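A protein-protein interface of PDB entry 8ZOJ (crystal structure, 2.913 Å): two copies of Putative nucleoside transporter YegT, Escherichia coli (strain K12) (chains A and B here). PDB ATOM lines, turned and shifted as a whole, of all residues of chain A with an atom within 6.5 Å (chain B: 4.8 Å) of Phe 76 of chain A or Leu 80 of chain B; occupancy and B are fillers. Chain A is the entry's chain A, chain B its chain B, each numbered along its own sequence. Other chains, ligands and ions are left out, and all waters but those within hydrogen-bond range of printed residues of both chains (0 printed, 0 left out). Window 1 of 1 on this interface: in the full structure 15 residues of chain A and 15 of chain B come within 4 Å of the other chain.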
ATOM      1  N   LEU A  71     -10.943   1.746   8.066  1.00  0.00           N
ATOM      2  CA  LEU A  71     -10.972   0.312   8.323  1.00  0.00           C
ATOM      3  C   LEU A  71     -12.362  -0.151   8.686  1.00  0.00           C
ATOM      4  O   LEU A  71     -12.800  -1.210   8.244  1.00  0.00           O
ATOM      5  CB  LEU A  71     -10.014  -0.051   9.448  1.00  0.00           C
ATOM      6  CG  LEU A  71      -9.937  -1.575   9.635  1.00  0.00           C
ATOM      7  CD1 LEU A  71      -8.548  -1.851  10.021  1.00  0.00           C
ATOM      8  CD2 LEU A  71     -10.898  -2.175  10.689  1.00  0.00           C
ATOM      9  N   ALA A  72     -13.020   0.571   9.584  1.00  0.00           N
ATOM     10  CA  ALA A  72     -14.415   0.278   9.871  1.00  0.00           C
ATOM     11  C   ALA A  72     -15.223   0.189   8.591  1.00  0.00           C
ATOM     12  O   ALA A  72     -15.991  -0.770   8.393  1.00  0.00           O
ATOM     13  CB  ALA A  72     -15.004   1.349  10.784  1.00  0.00           C
ATOM     14  N   VAL A  73     -15.046   1.167   7.695  1.00  0.00           N
ATOM     15  CA  VAL A  73     -15.789   1.139   6.430  1.00  0.00           C
ATOM     16  C   VAL A  73     -15.419  -0.096   5.606  1.00  0.00           C
ATOM     17  O   VAL A  73     -16.284  -0.739   5.002  1.00  0.00           O
ATOM     18  CB  VAL A  73     -15.577   2.449   5.638  1.00  0.00           C
ATOM     19  CG1 VAL A  73     -15.849   2.253   4.144  1.00  0.00           C
ATOM     20  CG2 VAL A  73     -16.501   3.527   6.165  1.00  0.00           C
ATOM     21  N   LEU A  74     -14.145  -0.465   5.584  1.00  0.00           N
ATOM     22  CA  LEU A  74     -13.748  -1.583   4.747  1.00  0.00           C
ATOM     23  C   LEU A  74     -14.224  -2.912   5.341  1.00  0.00           C
ATOM     24  O   LEU A  74     -14.669  -3.800   4.603  1.00  0.00           O
ATOM     25  CB  LEU A  74     -12.238  -1.572   4.529  1.00  0.00           C
ATOM     26  CG  LEU A  74     -11.742  -0.604   3.453  1.00  0.00           C
ATOM     27  CD1 LEU A  74     -10.350  -0.121   3.758  1.00  0.00           C
ATOM     28  CD2 LEU A  74     -11.729  -1.228   2.104  1.00  0.00           C
ATOM     29  N   MET A  75     -14.170  -3.071   6.668  1.00  0.00           N
ATOM     30  CA  MET A  75     -14.689  -4.299   7.263  1.00  0.00           C
ATOM     31  C   MET A  75     -16.176  -4.457   6.984  1.00  0.00           C
ATOM     32  O   MET A  75     -16.641  -5.561   6.650  1.00  0.00           O
ATOM     33  CB  MET A  75     -14.451  -4.353   8.768  1.00  0.00           C
ATOM     34  CG  MET A  75     -13.023  -4.585   9.221  1.00  0.00           C
ATOM     35  SD  MET A  75     -11.914  -5.662   8.286  1.00  0.00           S
ATOM     36  CE  MET A  75     -12.874  -7.115   8.094  1.00  0.00           C
ATOM     37  N   PHE A  76     -16.949  -3.376   7.135  1.00  0.00           N
ATOM     38  CA  PHE A  76     -18.363  -3.487   6.778  1.00  0.00           C
ATOM     39  C   PHE A  76     -18.530  -3.898   5.311  1.00  0.00           C
ATOM     40  O   PHE A  76     -19.304  -4.823   4.999  1.00  0.00           O
ATOM     41  CB  PHE A  76     -19.092  -2.176   7.070  1.00  0.00           C
ATOM     42  CG  PHE A  76     -19.057  -1.767   8.511  1.00  0.00           C
ATOM     43  CD1 PHE A  76     -18.552  -2.611   9.475  1.00  0.00           C
ATOM     44  CD2 PHE A  76     -19.549  -0.539   8.911  1.00  0.00           C
ATOM     45  CE1 PHE A  76     -18.526  -2.225  10.815  1.00  0.00           C
ATOM     46  CE2 PHE A  76     -19.519  -0.166  10.241  1.00  0.00           C
ATOM     47  CZ  PHE A  76     -19.002  -1.013  11.188  1.00  0.00           C
ATOM     48  N   ALA A  77     -17.792  -3.241   4.401  1.00  0.00           N
ATOM     49  CA  ALA A  77     -17.899  -3.593   2.992  1.00  0.00           C
ATOM     50  C   ALA A  77     -17.570  -5.064   2.772  1.00  0.00           C
ATOM     51  O   ALA A  77     -18.202  -5.735   1.943  1.00  0.00           O
ATOM     52  CB  ALA A  77     -16.987  -2.706   2.149  1.00  0.00           C
ATOM     53  N   GLY A  78     -16.594  -5.582   3.523  1.00  0.00           N
ATOM     54  CA  GLY A  78     -16.177  -6.967   3.342  1.00  0.00           C
ATOM     55  C   GLY A  78     -17.189  -7.960   3.888  1.00  0.00           C
ATOM     56  O   GLY A  78     -17.420  -9.020   3.295  1.00  0.00           O
ATOM     57  N   ALA A  79     -17.804  -7.628   5.025  1.00  0.00           N
ATOM     58  CA  ALA A  79     -18.918  -8.422   5.526  1.00  0.00           C
ATOM     59  C   ALA A  79     -19.980  -8.594   4.452  1.00  0.00           C
ATOM     60  O   ALA A  79     -20.399  -9.721   4.143  1.00  0.00           O
ATOM     61  CB  ALA A  79     -19.517  -7.764   6.766  1.00  0.00           C
ATOM     62  N   LEU A  80     -20.416  -7.476   3.865  1.00  0.00           N
ATOM     63  CA  LEU A  80     -21.466  -7.545   2.845  1.00  0.00           C
ATOM     64  C   LEU A  80     -21.013  -8.358   1.631  1.00  0.00           C
ATOM     65  O   LEU A  80     -21.743  -9.248   1.152  1.00  0.00           O
ATOM     66  CB  LEU A  80     -21.887  -6.128   2.433  1.00  0.00           C
ATOM     67  CG  LEU A  80     -22.957  -5.943   1.350  1.00  0.00           C
ATOM     68  CD1 LEU A  80     -23.748  -4.678   1.595  1.00  0.00           C
ATOM     69  CD2 LEU A  80     -22.336  -5.889  -0.040  1.00  0.00           C
ATOM     70  N   LEU A  81     -19.815  -8.072   1.124  1.00  0.00           N
ATOM     71  CA  LEU A  81     -19.353  -8.759  -0.068  1.00  0.00           C
ATOM     72  C   LEU A  81     -19.168 -10.253   0.183  1.00  0.00           C
ATOM     73  O   LEU A  81     -19.424 -11.088  -0.707  1.00  0.00           O
ATOM     74  CB  LEU A  81     -18.068  -8.105  -0.537  1.00  0.00           C
ATOM     75  CG  LEU A  81     -18.502  -6.749  -1.082  1.00  0.00           C
ATOM     76  CD1 LEU A  81     -17.296  -5.874  -1.452  1.00  0.00           C
ATOM     77  CD2 LEU A  81     -19.480  -6.953  -2.261  1.00  0.00           C
ATOM     78  N   THR A 104     -11.395  -5.329  -1.044  1.00  0.00           N
ATOM     79  CA  THR A 104     -11.693  -4.578   0.168  1.00  0.00           C
ATOM     80  C   THR A 104     -10.752  -4.996   1.280  1.00  0.00           C
ATOM     81  O   THR A 104     -10.292  -4.170   2.065  1.00  0.00           O
ATOM     82  CB  THR A 104     -13.145  -4.766   0.597  1.00  0.00           C
ATOM     83  OG1 THR A 104     -13.994  -3.925  -0.179  1.00  0.00           O
ATOM     84  CG2 THR A 104     -13.326  -4.322   1.998  1.00  0.00           C
ATOM     85  N   SER A 171     -15.608  -9.987  10.129  1.00  0.00           N
ATOM     86  CA  SER A 171     -15.478  -8.717   9.439  1.00  0.00           C
ATOM     87  C   SER A 171     -16.361  -7.678  10.094  1.00  0.00           C
ATOM     88  O   SER A 171     -15.912  -6.579  10.431  1.00  0.00           O
ATOM     89  CB  SER A 171     -15.850  -8.884   7.965  1.00  0.00           C
ATOM     90  OG  SER A 171     -14.715  -9.239   7.187  1.00  0.00           O
ATOM     91  N   ALA A 172     -17.624  -8.027  10.296  1.00  0.00           N
ATOM     92  CA  ALA A 172     -18.555  -7.122  10.949  1.00  0.00           C
ATOM     93  C   ALA A 172     -18.083  -6.777  12.356  1.00  0.00           C
ATOM     94  O   ALA A 172     -18.219  -5.626  12.799  1.00  0.00           O
ATOM     95  CB  ALA A 172     -19.946  -7.752  10.978  1.00  0.00           C
ATOM     96  N   LEU A 173     -17.507  -7.755  13.071  1.00  0.00           N
ATOM     97  CA  LEU A 173     -17.085  -7.495  14.447  1.00  0.00           C
ATOM     98  C   LEU A 173     -15.921  -6.504  14.491  1.00  0.00           C
ATOM     99  O   LEU A 173     -15.986  -5.488  15.190  1.00  0.00           O
ATOM    100  CB  LEU A 173     -16.699  -8.786  15.163  1.00  0.00           C
ATOM    101  CG  LEU A 173     -16.504  -8.521  16.666  1.00  0.00           C
ATOM    102  CD1 LEU A 173     -16.856  -9.712  17.479  1.00  0.00           C
ATOM    103  CD2 LEU A 173     -15.079  -8.093  17.026  1.00  0.00           C
ATOM    104  N   LEU A 174     -14.826  -6.828  13.800  1.00  0.00           N
ATOM    105  CA  LEU A 174     -13.693  -5.921  13.731  1.00  0.00           C
ATOM    106  C   LEU A 174     -14.116  -4.567  13.199  1.00  0.00           C
ATOM    107  O   LEU A 174     -13.604  -3.525  13.643  1.00  0.00           O
ATOM    108  CB  LEU A 174     -12.601  -6.508  12.853  1.00  0.00           C
ATOM    109  CG  LEU A 174     -11.456  -5.545  12.635  1.00  0.00           C
ATOM    110  CD1 LEU A 174     -10.860  -5.204  14.004  1.00  0.00           C
ATOM    111  CD2 LEU A 174     -10.416  -6.119  11.725  1.00  0.00           C
ATOM    112  N   GLY A 175     -15.063  -4.547  12.268  1.00  0.00           N
ATOM    113  CA  GLY A 175     -15.623  -3.277  11.859  1.00  0.00           C
ATOM    114  C   GLY A 175     -16.138  -2.474  13.032  1.00  0.00           C
ATOM    115  O   GLY A 175     -15.662  -1.371  13.294  1.00  0.00           O
ATOM    116  N   VAL A 176     -17.081  -3.038  13.785  1.00  0.00           N
ATOM    117  CA  VAL A 176     -17.613  -2.293  14.924  1.00  0.00           C
ATOM    118  C   VAL A 176     -16.518  -1.967  15.940  1.00  0.00           C
ATOM    119  O   VAL A 176     -16.520  -0.880  16.529  1.00  0.00           O
ATOM    120  CB  VAL A 176     -18.778  -3.054  15.578  1.00  0.00           C
ATOM    121  CG1 VAL A 176     -19.120  -2.445  16.925  1.00  0.00           C
ATOM    122  CG2 VAL A 176     -20.002  -3.015  14.667  1.00  0.00           C
ATOM    123  N   PHE A 177     -15.569  -2.887  16.157  1.00  0.00           N
ATOM    124  CA  PHE A 177     -14.474  -2.678  17.103  1.00  0.00           C
ATOM    125  C   PHE A 177     -13.562  -1.532  16.673  1.00  0.00           C
ATOM    126  O   PHE A 177     -12.804  -0.999  17.493  1.00  0.00           O
ATOM    127  CB  PHE A 177     -13.675  -3.969  17.265  1.00  0.00           C
ATOM    128  CG  PHE A 177     -12.514  -3.851  18.206  1.00  0.00           C
ATOM    129  CD1 PHE A 177     -12.719  -3.632  19.547  1.00  0.00           C
ATOM    130  CD2 PHE A 177     -11.215  -3.955  17.739  1.00  0.00           C
ATOM    131  CE1 PHE A 177     -11.640  -3.518  20.414  1.00  0.00           C
ATOM    132  CE2 PHE A 177     -10.135  -3.843  18.597  1.00  0.00           C
ATOM    133  CZ  PHE A 177     -10.345  -3.625  19.937  1.00  0.00           C
ATOM    134  N   PHE A 179     -14.587   1.381  16.050  1.00  0.00           N
ATOM    135  CA  PHE A 179     -15.031   2.623  16.691  1.00  0.00           C
ATOM    136  C   PHE A 179     -14.139   2.958  17.882  1.00  0.00           C
ATOM    137  O   PHE A 179     -13.663   4.088  18.014  1.00  0.00           O
ATOM    138  CB  PHE A 179     -16.486   2.542  17.181  1.00  0.00           C
ATOM    139  CG  PHE A 179     -17.487   2.027  16.176  1.00  0.00           C
ATOM    140  CD1 PHE A 179     -17.194   1.913  14.826  1.00  0.00           C
ATOM    141  CD2 PHE A 179     -18.765   1.688  16.605  1.00  0.00           C
ATOM    142  CE1 PHE A 179     -18.153   1.431  13.926  1.00  0.00           C
ATOM    143  CE2 PHE A 179     -19.720   1.221  15.724  1.00  0.00           C
ATOM    144  CZ  PHE A 179     -19.415   1.095  14.378  1.00  0.00           C
ATOM    145  N   PHE B  76     -25.692  -4.662   6.579  1.00  0.00           N
ATOM    146  CA  PHE B  76     -24.283  -4.323   6.402  1.00  0.00           C
ATOM    147  C   PHE B  76     -24.113  -2.970   5.687  1.00  0.00           C
ATOM    148  O   PHE B  76     -23.380  -2.093   6.179  1.00  0.00           O
ATOM    149  CB  PHE B  76     -23.562  -5.441   5.657  1.00  0.00           C
ATOM    150  CG  PHE B  76     -23.454  -6.712   6.434  1.00  0.00           C
ATOM    151  CD1 PHE B  76     -23.198  -6.688   7.789  1.00  0.00           C
ATOM    152  CD2 PHE B  76     -23.611  -7.946   5.803  1.00  0.00           C
ATOM    153  CE1 PHE B  76     -23.104  -7.891   8.517  1.00  0.00           C
ATOM    154  CE2 PHE B  76     -23.522  -9.137   6.519  1.00  0.00           C
ATOM    155  CZ  PHE B  76     -23.274  -9.107   7.875  1.00  0.00           C
ATOM    156  N   ALA B  77     -24.789  -2.775   4.543  1.00  0.00           N
ATOM    157  CA  ALA B  77     -24.738  -1.472   3.884  1.00  0.00           C
ATOM    158  C   ALA B  77     -25.138  -0.351   4.834  1.00  0.00           C
ATOM    159  O   ALA B  77     -24.539   0.728   4.809  1.00  0.00           O
ATOM    160  CB  ALA B  77     -25.634  -1.444   2.648  1.00  0.00           C
ATOM    161  N   GLY B  78     -26.155  -0.568   5.669  1.00  0.00           N
ATOM    162  CA  GLY B  78     -26.587   0.507   6.556  1.00  0.00           C
ATOM    163  C   GLY B  78     -25.539   0.886   7.596  1.00  0.00           C
ATOM    164  O   GLY B  78     -25.290   2.072   7.846  1.00  0.00           O
ATOM    165  N   ALA B  79     -24.929  -0.124   8.222  1.00  0.00           N
ATOM    166  CA  ALA B  79     -23.813   0.089   9.131  1.00  0.00           C
ATOM    167  C   ALA B  79     -22.719   0.911   8.472  1.00  0.00           C
ATOM    168  O   ALA B  79     -22.252   1.910   9.032  1.00  0.00           O
ATOM    169  CB  ALA B  79     -23.261  -1.257   9.576  1.00  0.00           C
ATOM    170  N   LEU B  80     -22.300   0.507   7.270  1.00  0.00           N
ATOM    171  CA  LEU B  80     -21.269   1.253   6.536  1.00  0.00           C
ATOM    172  C   LEU B  80     -21.699   2.697   6.257  1.00  0.00           C
ATOM    173  O   LEU B  80     -20.997   3.658   6.613  1.00  0.00           O
ATOM    174  CB  LEU B  80     -20.965   0.526   5.224  1.00  0.00           C
ATOM    175  CG  LEU B  80     -19.837   0.912   4.264  1.00  0.00           C
ATOM    176  CD1 LEU B  80     -19.744  -0.156   3.157  1.00  0.00           C
ATOM    177  CD2 LEU B  80     -20.044   2.274   3.658  1.00  0.00           C
ATOM    178  N   LEU B  81     -22.829   2.851   5.573  1.00  0.00           N
ATOM    179  CA  LEU B  81     -23.315   4.150   5.149  1.00  0.00           C
ATOM    180  C   LEU B  81     -23.450   5.108   6.323  1.00  0.00           C
ATOM    181  O   LEU B  81     -23.069   6.288   6.231  1.00  0.00           O
ATOM    182  CB  LEU B  81     -24.651   3.961   4.448  1.00  0.00           C
ATOM    183  CG  LEU B  81     -24.399   3.720   2.970  1.00  0.00           C
ATOM    184  CD1 LEU B  81     -25.729   3.499   2.274  1.00  0.00           C
ATOM    185  CD2 LEU B  81     -23.589   4.910   2.375  1.00  0.00           C
ATOM    186  N   MET B  82     -23.969   4.633   7.448  1.00  0.00           N
ATOM    187  CA  MET B  82     -24.138   5.620   8.488  1.00  0.00           C
ATOM    188  C   MET B  82     -22.876   5.839   9.292  1.00  0.00           C
ATOM    189  O   MET B  82     -22.717   6.919   9.842  1.00  0.00           O
ATOM    190  CB  MET B  82     -25.270   5.282   9.433  1.00  0.00           C
ATOM    191  CG  MET B  82     -25.602   6.515  10.238  1.00  0.00           C
ATOM    192  SD  MET B  82     -26.609   6.095  11.612  1.00  0.00           S
ATOM    193  CE  MET B  82     -28.230   6.201  10.839  1.00  0.00           C
ATOM    194  N   TYR B  83     -21.971   4.865   9.397  1.00  0.00           N
ATOM    195  CA  TYR B  83     -20.674   5.193   9.976  1.00  0.00           C
ATOM    196  C   TYR B  83     -20.064   6.366   9.222  1.00  0.00           C
ATOM    197  O   TYR B  83     -19.722   7.417   9.807  1.00  0.00           O
ATOM    198  CB  TYR B  83     -19.751   3.970   9.931  1.00  0.00           C
ATOM    199  CG  TYR B  83     -18.420   4.208  10.598  1.00  0.00           C
ATOM    200  CD1 TYR B  83     -18.271   4.005  11.963  1.00  0.00           C
ATOM    201  CD2 TYR B  83     -17.321   4.687   9.880  1.00  0.00           C
ATOM    202  CE1 TYR B  83     -17.067   4.253  12.604  1.00  0.00           C
ATOM    203  CE2 TYR B  83     -16.101   4.931  10.505  1.00  0.00           C
ATOM    204  CZ  TYR B  83     -15.980   4.710  11.874  1.00  0.00           C
ATOM    205  OH  TYR B  83     -14.780   4.946  12.529  1.00  0.00           O
ATOM    206  N   PHE B  84     -20.002   6.215   7.896  1.00  0.00           N
ATOM    207  CA  PHE B  84     -19.589   7.302   7.014  1.00  0.00           C
ATOM    208  C   PHE B  84     -20.322   8.612   7.337  1.00  0.00           C
ATOM    209  O   PHE B  84     -19.697   9.669   7.460  1.00  0.00           O
ATOM    210  CB  PHE B  84     -19.833   6.881   5.559  1.00  0.00           C
ATOM    211  CG  PHE B  84     -18.762   7.336   4.596  1.00  0.00           C
ATOM    212  CD1 PHE B  84     -17.578   6.643   4.489  1.00  0.00           C
ATOM    213  CD2 PHE B  84     -18.957   8.435   3.783  1.00  0.00           C
ATOM    214  CE1 PHE B  84     -16.617   7.040   3.592  1.00  0.00           C
ATOM    215  CE2 PHE B  84     -18.003   8.840   2.892  1.00  0.00           C
ATOM    216  CZ  PHE B  84     -16.823   8.146   2.795  1.00  0.00           C
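Among the printed residues, pairs that only touch across the chains: Phe 179 of chain A with Tyr 83 of chain B (3.2 Å), Phe 76 of chain A with Leu 80 of chain B (3.4 Å), Phe 76 of chain A with Ala 79 of chain B (3.5 Å), Leu 80 of chain A with Ala 77 of chain B (3.7 Å), Ala 72 of chain A with Tyr 83 of chain B (3.7 Å), Leu 80 of chain A with Phe 76 of chain B (3.7 Å), Val 73 of chain A with Phe 84 of chain B (3.7 Å), Ala 77 of chain A with Leu 80 of chain B (3.9 Å), Ala 79 of chain A with Phe 76 of chain B (3.9 Å), Val 73 of chain A with Leu 80 of chain B (3.96 Å) and Val 73 of chain A with Tyr 83 of chain B (3.98 Å).
Of chain B, only Ala 79 and Leu 80 come within 4 Å of Phe 76 of chain A.
Of chain A, only Val 73, Phe 76 and Ala 77 come within 4 Å of Leu 80 of chain B.
Printed residues of chain A within 4 Å of Phe 76 of chain B: Ala 79 (3.9 Å) and Leu 80 (3.7 Å).
Of the printed residues of chain A, Tyr 83 of chain B touches Ala 72 (3.7 Å), Val 73 (3.98 Å) and Phe 179 (3.2 Å).
Of the printed residues of chain A, Phe 84 of chain B touches Val 73 (3.7 Å).
The nearest residue of chain A that does not touch Leu 80 of chain B is Ala 72 of chain A (5.9 Å).
The nearest printed residue of chain B that does not touch Phe 179 of chain A is Ala 79 of chain B (6.1 Å).
Hydrophobic or aromatic side chains of chain A that line the printed part of chain B: Ala 72, Val 73, Phe 76, Ala 77, Ala 79, Leu 80 and Phe 179.
Of the 9 printed residues of chain B, 6 touch a printed residue of chain A.
Among the printed residues, 11 pairs touch across the chains.
Phe 76 of chain A touches Ala 79 of chain B, and with the chains exchanged Ala 79 of chain A touches Phe 76 of chain B.
Phe 76 of chain A touches Leu 80 of chain B, and with the chains exchanged Leu 80 of chain A touches Phe 76 of chain B.
Ala 77 of chain A touches Leu 80 of chain B, and with the chains exchanged Leu 80 of chain A touches Ala 77 of chain B.
Positions printed for both chains: 76, 77, 78, 79, 80 and 81.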
